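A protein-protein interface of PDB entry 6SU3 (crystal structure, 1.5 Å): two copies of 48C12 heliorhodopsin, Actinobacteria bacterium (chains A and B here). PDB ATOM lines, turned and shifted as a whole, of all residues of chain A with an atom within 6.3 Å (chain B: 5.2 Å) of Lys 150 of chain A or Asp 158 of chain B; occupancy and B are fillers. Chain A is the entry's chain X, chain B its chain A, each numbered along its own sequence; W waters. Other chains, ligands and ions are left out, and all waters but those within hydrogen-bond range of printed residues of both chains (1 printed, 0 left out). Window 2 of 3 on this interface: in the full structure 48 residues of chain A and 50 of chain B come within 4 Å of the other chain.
Hydrophobic or aromatic side chains of chain A that line the printed part of chain B: Trp 146, Leu 147 and Tyr 151. Along chain B the printed residues that touch a printed residue of chain A span positions 152 to 161. Among the printed residues, 7 pairs touch across the chains.
Water W1 lies within hydrogen-bond range of OD1 of Asp 158 of chain B and NZ of Lys 150 of chain A.
OD2 of Asp 158 of chain B sits at hydrogen-bond distance from OH of Tyr 151 of chain A.
Among the printed residues, merely in contact across the chains: Trp 146 of chain A with Leu 160 of chain B (3.7 Å), Leu 147 of chain A with Pro 161 of chain B (3.9 Å), Lys 150 of chain A with Asp 158 of chain B (3.4 Å), Lys 150 of chain A with Leu 160 of chain B (3.7 Å), Tyr 151 of chain A with Thr 152 of chain B (3.8 Å) and Tyr 151 of chain A with Pro 161 of chain B (3.2 Å).
Of chain A, only Lys 150 and Tyr 151 come within 4 Å of Asp 158 of chain B. Of the printed residues of chain B, Trp 146 of chain A touches Leu 160 (3.7 Å). Of the printed residues of chain A, Leu 160 of chain B touches Trp 146 and Lys 150. Of the printed residues of chain B, Tyr 151 of chain A touches Thr 152 (3.8 Å), Asp 158 (2.6 Å) and Pro 161 (3.2 Å). Printed residues of chain A within 4 Å of Thr 152 of chain B: Tyr 151. Of the printed residues of chain A, Pro 161 of chain B touches Leu 147 (3.9 Å) and Tyr 151 (3.2 Å). Gly 145 of chain A touches none of the printed residues of chain B. Gln 100 of chain A touches none of the printed residues of chain B. The nearest printed residue of chain B that does not touch Lys 150 of chain A is Pro 161 of chain B (5.6 Å).
2 positions are printed for both chains. Of the 7 pairs that touch across the chains among the printed residues, none has its exchanged pair printed and touching as well.
The backbone carbonyl oxygen (O) of Asp 158 of chain B is in hydrogen-bond range of the side-chain amide nitrogen (NE2) of Gln 148 of chain B. O of Gln 148 of chain B sits at hydrogen-bond distance from OG1 of Thr 152 of chain B (2.7 Å). The side-chain carboxylate (OD1) of Asp 156 of chain B is in hydrogen-bond range of the backbone NH (N) of Asp 158 of chain B. The backbone NH (N) of Leu 160 of chain B sits at hydrogen-bond distance from the side-chain carboxylate (OD1) of Asp 158 of chain B (3.1 Å).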
ATOM      1  N   ASN A  99       8.552 -31.841  27.359  1.00  0.00           N
ATOM      2  CA  ASN A  99       8.399 -31.271  28.723  1.00  0.00           C
ATOM      3  C   ASN A  99       8.924 -29.833  28.732  1.00  0.00           C
ATOM      4  O   ASN A  99       9.727 -29.492  29.630  1.00  0.00           O
ATOM      5  CB  ASN A  99       9.095 -32.142  29.770  1.00  0.00           C
ATOM      6  CG  ASN A  99       8.554 -33.553  29.790  1.00  0.00           C
ATOM      7  OD1 ASN A  99       7.346 -33.746  29.900  1.00  0.00           O
ATOM      8  ND2 ASN A  99       9.431 -34.535  29.655  1.00  0.00           N
ATOM      9  N   GLN A 100       8.485 -29.020  27.767  1.00  0.00           N
ATOM     10  CA  GLN A 100       8.896 -27.599  27.642  1.00  0.00           C
ATOM     11  C   GLN A 100       7.662 -26.731  27.420  1.00  0.00           C
ATOM     12  O   GLN A 100       6.744 -27.175  26.705  1.00  0.00           O
ATOM     13  CB  GLN A 100       9.836 -27.399  26.453  1.00  0.00           C
ATOM     14  CG  GLN A 100      11.162 -28.116  26.593  1.00  0.00           C
ATOM     15  CD  GLN A 100      12.036 -27.834  25.400  1.00  0.00           C
ATOM     16  OE1 GLN A 100      11.808 -26.881  24.664  1.00  0.00           O
ATOM     17  NE2 GLN A 100      13.048 -28.662  25.204  1.00  0.00           N
ATOM     18  N   ILE A 102       8.094 -22.801  26.328  1.00  0.00           N
ATOM     19  CA  ILE A 102       9.052 -21.680  26.138  1.00  0.00           C
ATOM     20  C   ILE A 102       8.284 -20.353  26.218  1.00  0.00           C
ATOM     21  O   ILE A 102       8.849 -19.378  26.713  1.00  0.00           O
ATOM     22  CB  ILE A 102       9.838 -21.849  24.827  1.00  0.00           C
ATOM     23  CG1 ILE A 102      10.629 -23.162  24.811  1.00  0.00           C
ATOM     24  CG2 ILE A 102      10.726 -20.646  24.576  1.00  0.00           C
ATOM     25  CD1 ILE A 102      11.183 -23.579  26.158  1.00  0.00           C
ATOM     26  N   GLY A 145      15.373 -21.103  34.521  1.00  0.00           N
ATOM     27  CA  GLY A 145      14.233 -22.032  34.465  1.00  0.00           C
ATOM     28  C   GLY A 145      14.004 -22.520  33.046  1.00  0.00           C
ATOM     29  O   GLY A 145      13.731 -23.706  32.853  1.00  0.00           O
ATOM     30  N   TRP A 146      14.129 -21.624  32.070  1.00  0.00           N
ATOM     31  CA  TRP A 146      14.031 -21.959  30.630  1.00  0.00           C
ATOM     32  C   TRP A 146      15.124 -22.983  30.280  1.00  0.00           C
ATOM     33  O   TRP A 146      14.810 -24.013  29.667  1.00  0.00           O
ATOM     34  CB  TRP A 146      14.115 -20.651  29.846  1.00  0.00           C
ATOM     35  CG  TRP A 146      14.120 -20.707  28.353  1.00  0.00           C
ATOM     36  CD1 TRP A 146      14.392 -21.753  27.518  1.00  0.00           C
ATOM     37  CD2 TRP A 146      13.905 -19.568  27.507  1.00  0.00           C
ATOM     38  NE1 TRP A 146      14.343 -21.341  26.208  1.00  0.00           N
ATOM     39  CE2 TRP A 146      14.043 -20.005  26.172  1.00  0.00           C
ATOM     40  CE3 TRP A 146      13.583 -18.230  27.756  1.00  0.00           C
ATOM     41  CZ2 TRP A 146      13.875 -19.136  25.096  1.00  0.00           C
ATOM     42  CZ3 TRP A 146      13.434 -17.373  26.693  1.00  0.00           C
ATOM     43  CH2 TRP A 146      13.574 -17.826  25.384  1.00  0.00           C
ATOM     44  N   LEU A 147      16.363 -22.755  30.720  1.00  0.00           N
ATOM     45  CA  LEU A 147      17.491 -23.681  30.421  1.00  0.00           C
ATOM     46  C   LEU A 147      17.293 -25.027  31.136  1.00  0.00           C
ATOM     47  O   LEU A 147      17.689 -26.057  30.558  1.00  0.00           O
ATOM     48  CB  LEU A 147      18.812 -23.010  30.800  1.00  0.00           C
ATOM     49  CG  LEU A 147      19.182 -21.787  29.960  1.00  0.00           C
ATOM     50  CD1 LEU A 147      20.631 -21.388  30.195  1.00  0.00           C
ATOM     51  CD2 LEU A 147      18.940 -22.033  28.480  1.00  0.00           C
ATOM     52  N   GLN A 148      16.705 -25.052  32.336  1.00  0.00           N
ATOM     53  CA  GLN A 148      16.319 -26.327  32.999  1.00  0.00           C
ATOM     54  C   GLN A 148      15.449 -27.135  32.027  1.00  0.00           C
ATOM     55  O   GLN A 148      15.741 -28.338  31.817  1.00  0.00           O
ATOM     56  CB  GLN A 148      15.622 -26.078  34.337  1.00  0.00           C
ATOM     57  CG  GLN A 148      15.171 -27.346  35.049  1.00  0.00           C
ATOM     58  CD  GLN A 148      16.285 -28.131  35.703  1.00  0.00           C
ATOM     59  OE1 GLN A 148      17.275 -27.577  36.169  1.00  0.00           O
ATOM     60  NE2 GLN A 148      16.116 -29.445  35.776  1.00  0.00           N
ATOM     61  N   GLU A 149      14.433 -26.505  31.436  1.00  0.00           N
ATOM     62  CA  GLU A 149      13.494 -27.194  30.511  1.00  0.00           C
ATOM     63  C   GLU A 149      14.217 -27.549  29.210  1.00  0.00           C
ATOM     64  O   GLU A 149      13.911 -28.605  28.642  1.00  0.00           O
ATOM     65  CB  GLU A 149      12.269 -26.325  30.231  1.00  0.00           C
ATOM     66  CG  GLU A 149      11.410 -26.091  31.459  1.00  0.00           C
ATOM     67  CD  GLU A 149       9.928 -26.040  31.148  1.00  0.00           C
ATOM     68  OE1 GLU A 149       9.550 -25.386  30.159  1.00  0.00           O
ATOM     69  OE2 GLU A 149       9.171 -26.662  31.887  1.00  0.00           O
ATOM     70  N   LYS A 150      15.110 -26.689  28.715  1.00  0.00           N
ATOM     71  CA  LYS A 150      15.737 -26.918  27.385  1.00  0.00           C
ATOM     72  C   LYS A 150      16.645 -28.155  27.457  1.00  0.00           C
ATOM     73  O   LYS A 150      16.612 -28.966  26.510  1.00  0.00           O
ATOM     74  CB  LYS A 150      16.507 -25.689  26.900  1.00  0.00           C
ATOM     75  CG  LYS A 150      17.068 -25.822  25.492  1.00  0.00           C
ATOM     76  CD  LYS A 150      17.778 -24.576  25.020  1.00  0.00           C
ATOM     77  CE  LYS A 150      18.475 -24.747  23.688  1.00  0.00           C
ATOM     78  NZ  LYS A 150      17.531 -24.522  22.578  1.00  0.00           N
ATOM     79  N   TYR A 151      17.411 -28.324  28.537  1.00  0.00           N
ATOM     80  CA  TYR A 151      18.580 -29.238  28.559  1.00  0.00           C
ATOM     81  C   TYR A 151      18.365 -30.458  29.461  1.00  0.00           C
ATOM     82  O   TYR A 151      19.175 -31.378  29.355  1.00  0.00           O
ATOM     83  CB  TYR A 151      19.845 -28.483  28.956  1.00  0.00           C
ATOM     84  CG  TYR A 151      20.261 -27.456  27.937  1.00  0.00           C
ATOM     85  CD1 TYR A 151      20.516 -27.802  26.621  1.00  0.00           C
ATOM     86  CD2 TYR A 151      20.371 -26.124  28.290  1.00  0.00           C
ATOM     87  CE1 TYR A 151      20.879 -26.847  25.683  1.00  0.00           C
ATOM     88  CE2 TYR A 151      20.724 -25.166  27.365  1.00  0.00           C
ATOM     89  CZ  TYR A 151      20.990 -25.521  26.058  1.00  0.00           C
ATOM     90  OH  TYR A 151      21.332 -24.536  25.166  1.00  0.00           O
ATOM     91  N   THR A 152      17.342 -30.478  30.310  1.00  0.00           N
ATOM     92  CA  THR A 152      17.080 -31.609  31.236  1.00  0.00           C
ATOM     93  C   THR A 152      15.703 -32.229  30.965  1.00  0.00           C
ATOM     94  O   THR A 152      14.894 -31.638  30.239  1.00  0.00           O
ATOM     95  CB  THR A 152      17.222 -31.205  32.706  1.00  0.00           C
ATOM     96  OG1 THR A 152      15.990 -30.586  33.082  1.00  0.00           O
ATOM     97  CG2 THR A 152      18.407 -30.295  32.962  1.00  0.00           C
ATOM     98  N   GLN A 153      15.470 -33.412  31.523  1.00  0.00           N
ATOM     99  CA  GLN A 153      14.129 -34.048  31.554  1.00  0.00           C
ATOM    100  C   GLN A 153      13.837 -34.441  32.997  1.00  0.00           C
ATOM    101  O   GLN A 153      14.754 -34.705  33.776  1.00  0.00           O
ATOM    102  CB  GLN A 153      14.054 -35.244  30.597  1.00  0.00           C
ATOM    103  CG  GLN A 153      14.102 -34.858  29.126  1.00  0.00           C
ATOM    104  CD  GLN A 153      12.919 -34.028  28.689  1.00  0.00           C
ATOM    105  OE1 GLN A 153      12.057 -33.669  29.484  1.00  0.00           O
ATOM    106  NE2 GLN A 153      12.878 -33.704  27.408  1.00  0.00           N
ATOM    107  N   TYR A 217      10.520 -31.717  37.894  1.00  0.00           N
ATOM    108  CA  TYR A 217      11.812 -32.293  37.430  1.00  0.00           C
ATOM    109  C   TYR A 217      12.258 -33.401  38.389  1.00  0.00           C
ATOM    110  O   TYR A 217      12.976 -34.334  37.942  1.00  0.00           O
ATOM    111  CB  TYR A 217      12.815 -31.175  37.118  1.00  0.00           C
ATOM    112  CG  TYR A 217      12.531 -30.633  35.744  1.00  0.00           C
ATOM    113  CD1 TYR A 217      13.187 -31.142  34.637  1.00  0.00           C
ATOM    114  CD2 TYR A 217      11.478 -29.758  35.525  1.00  0.00           C
ATOM    115  CE1 TYR A 217      12.857 -30.736  33.358  1.00  0.00           C
ATOM    116  CE2 TYR A 217      11.135 -29.344  34.250  1.00  0.00           C
ATOM    117  CZ  TYR A 217      11.821 -29.844  33.160  1.00  0.00           C
ATOM    118  OH  TYR A 217      11.498 -29.468  31.895  1.00  0.00           O
ATOM    119  N   GLN B 148      26.433 -22.970  29.149  1.00  0.00           N
ATOM    120  CA  GLN B 148      26.861 -23.081  27.729  1.00  0.00           C
ATOM    121  C   GLN B 148      27.820 -24.273  27.600  1.00  0.00           C
ATOM    122  O   GLN B 148      27.623 -25.110  26.705  1.00  0.00           O
ATOM    123  CB  GLN B 148      27.497 -21.778  27.247  1.00  0.00           C
ATOM    124  CG  GLN B 148      28.011 -21.832  25.816  1.00  0.00           C
ATOM    125  CD  GLN B 148      26.923 -21.817  24.776  1.00  0.00           C
ATOM    126  OE1 GLN B 148      25.910 -21.141  24.931  1.00  0.00           O
ATOM    127  NE2 GLN B 148      27.128 -22.576  23.698  1.00  0.00           N
ATOM    128  N   THR B 152      26.146 -27.806  25.769  1.00  0.00           N
ATOM    129  CA  THR B 152      26.362 -27.644  24.309  1.00  0.00           C
ATOM    130  C   THR B 152      27.766 -28.120  23.940  1.00  0.00           C
ATOM    131  O   THR B 152      28.639 -28.240  24.825  1.00  0.00           O
ATOM    132  CB  THR B 152      26.107 -26.213  23.821  1.00  0.00           C
ATOM    133  OG1 THR B 152      27.294 -25.452  24.054  1.00  0.00           O
ATOM    134  CG2 THR B 152      24.913 -25.546  24.472  1.00  0.00           C
ATOM    135  N   ASP B 156      27.900 -26.884  17.392  1.00  0.00           N
ATOM    136  CA  ASP B 156      26.534 -27.478  17.406  1.00  0.00           C
ATOM    137  C   ASP B 156      25.489 -26.418  17.043  1.00  0.00           C
ATOM    138  O   ASP B 156      24.341 -26.811  16.797  1.00  0.00           O
ATOM    139  CB  ASP B 156      26.212 -28.153  18.739  1.00  0.00           C
ATOM    140  CG  ASP B 156      25.719 -27.211  19.832  1.00  0.00           C
ATOM    141  OD1 ASP B 156      25.802 -25.969  19.649  1.00  0.00           O
ATOM    142  OD2 ASP B 156      25.268 -27.726  20.874  1.00  0.00           O
ATOM    143  N   GLY B 157      25.860 -25.133  17.006  1.00  0.00           N
ATOM    144  CA  GLY B 157      24.986 -24.041  16.532  1.00  0.00           C
ATOM    145  C   GLY B 157      24.074 -23.520  17.636  1.00  0.00           C
ATOM    146  O   GLY B 157      23.202 -22.677  17.349  1.00  0.00           O
ATOM    147  N   ASP B 158      24.267 -23.991  18.868  1.00  0.00           N
ATOM    148  CA  ASP B 158      23.442 -23.585  20.037  1.00  0.00           C
ATOM    149  C   ASP B 158      24.265 -22.642  20.926  1.00  0.00           C
ATOM    150  O   ASP B 158      25.203 -23.113  21.595  1.00  0.00           O
ATOM    151  CB  ASP B 158      22.939 -24.809  20.805  1.00  0.00           C
ATOM    152  CG  ASP B 158      22.023 -24.477  21.969  1.00  0.00           C
ATOM    153  OD1 ASP B 158      21.662 -23.274  22.126  1.00  0.00           O
ATOM    154  OD2 ASP B 158      21.696 -25.411  22.722  1.00  0.00           O
ATOM    155  N   LEU B 159      23.906 -21.359  20.925  1.00  0.00           N
ATOM    156  CA  LEU B 159      24.536 -20.320  21.778  1.00  0.00           C
ATOM    157  C   LEU B 159      23.495 -19.737  22.740  1.00  0.00           C
ATOM    158  O   LEU B 159      23.709 -18.631  23.218  1.00  0.00           O
ATOM    159  CB  LEU B 159      25.123 -19.230  20.879  1.00  0.00           C
ATOM    160  CG  LEU B 159      26.433 -19.573  20.180  1.00  0.00           C
ATOM    161  CD1 LEU B 159      26.793 -18.494  19.168  1.00  0.00           C
ATOM    162  CD2 LEU B 159      27.555 -19.758  21.179  1.00  0.00           C
ATOM    163  N   LEU B 160      22.396 -20.438  23.023  1.00  0.00           N
ATOM    164  CA  LEU B 160      21.312 -19.791  23.810  1.00  0.00           C
ATOM    165  C   LEU B 160      21.830 -19.390  25.192  1.00  0.00           C
ATOM    166  O   LEU B 160      21.617 -18.260  25.612  1.00  0.00           O
ATOM    167  CB  LEU B 160      20.068 -20.669  23.914  1.00  0.00           C
ATOM    168  CG  LEU B 160      18.871 -19.939  24.527  1.00  0.00           C
ATOM    169  CD1 LEU B 160      18.414 -18.801  23.628  1.00  0.00           C
ATOM    170  CD2 LEU B 160      17.729 -20.902  24.801  1.00  0.00           C
ATOM    171  N   PRO B 161      22.508 -20.273  25.960  1.00  0.00           N
ATOM    172  CA  PRO B 161      23.023 -19.876  27.273  1.00  0.00           C
ATOM    173  C   PRO B 161      23.997 -18.693  27.181  1.00  0.00           C
ATOM    174  O   PRO B 161      23.914 -17.776  27.995  1.00  0.00           O
ATOM    175  CB  PRO B 161      23.702 -21.151  27.801  1.00  0.00           C
ATOM    176  CG  PRO B 161      23.027 -22.265  27.032  1.00  0.00           C
ATOM    177  CD  PRO B 161      22.767 -21.687  25.659  1.00  0.00           C
HETATM  178  O   HOH W   1      19.282 -22.783  20.935  1.00  0.00           O
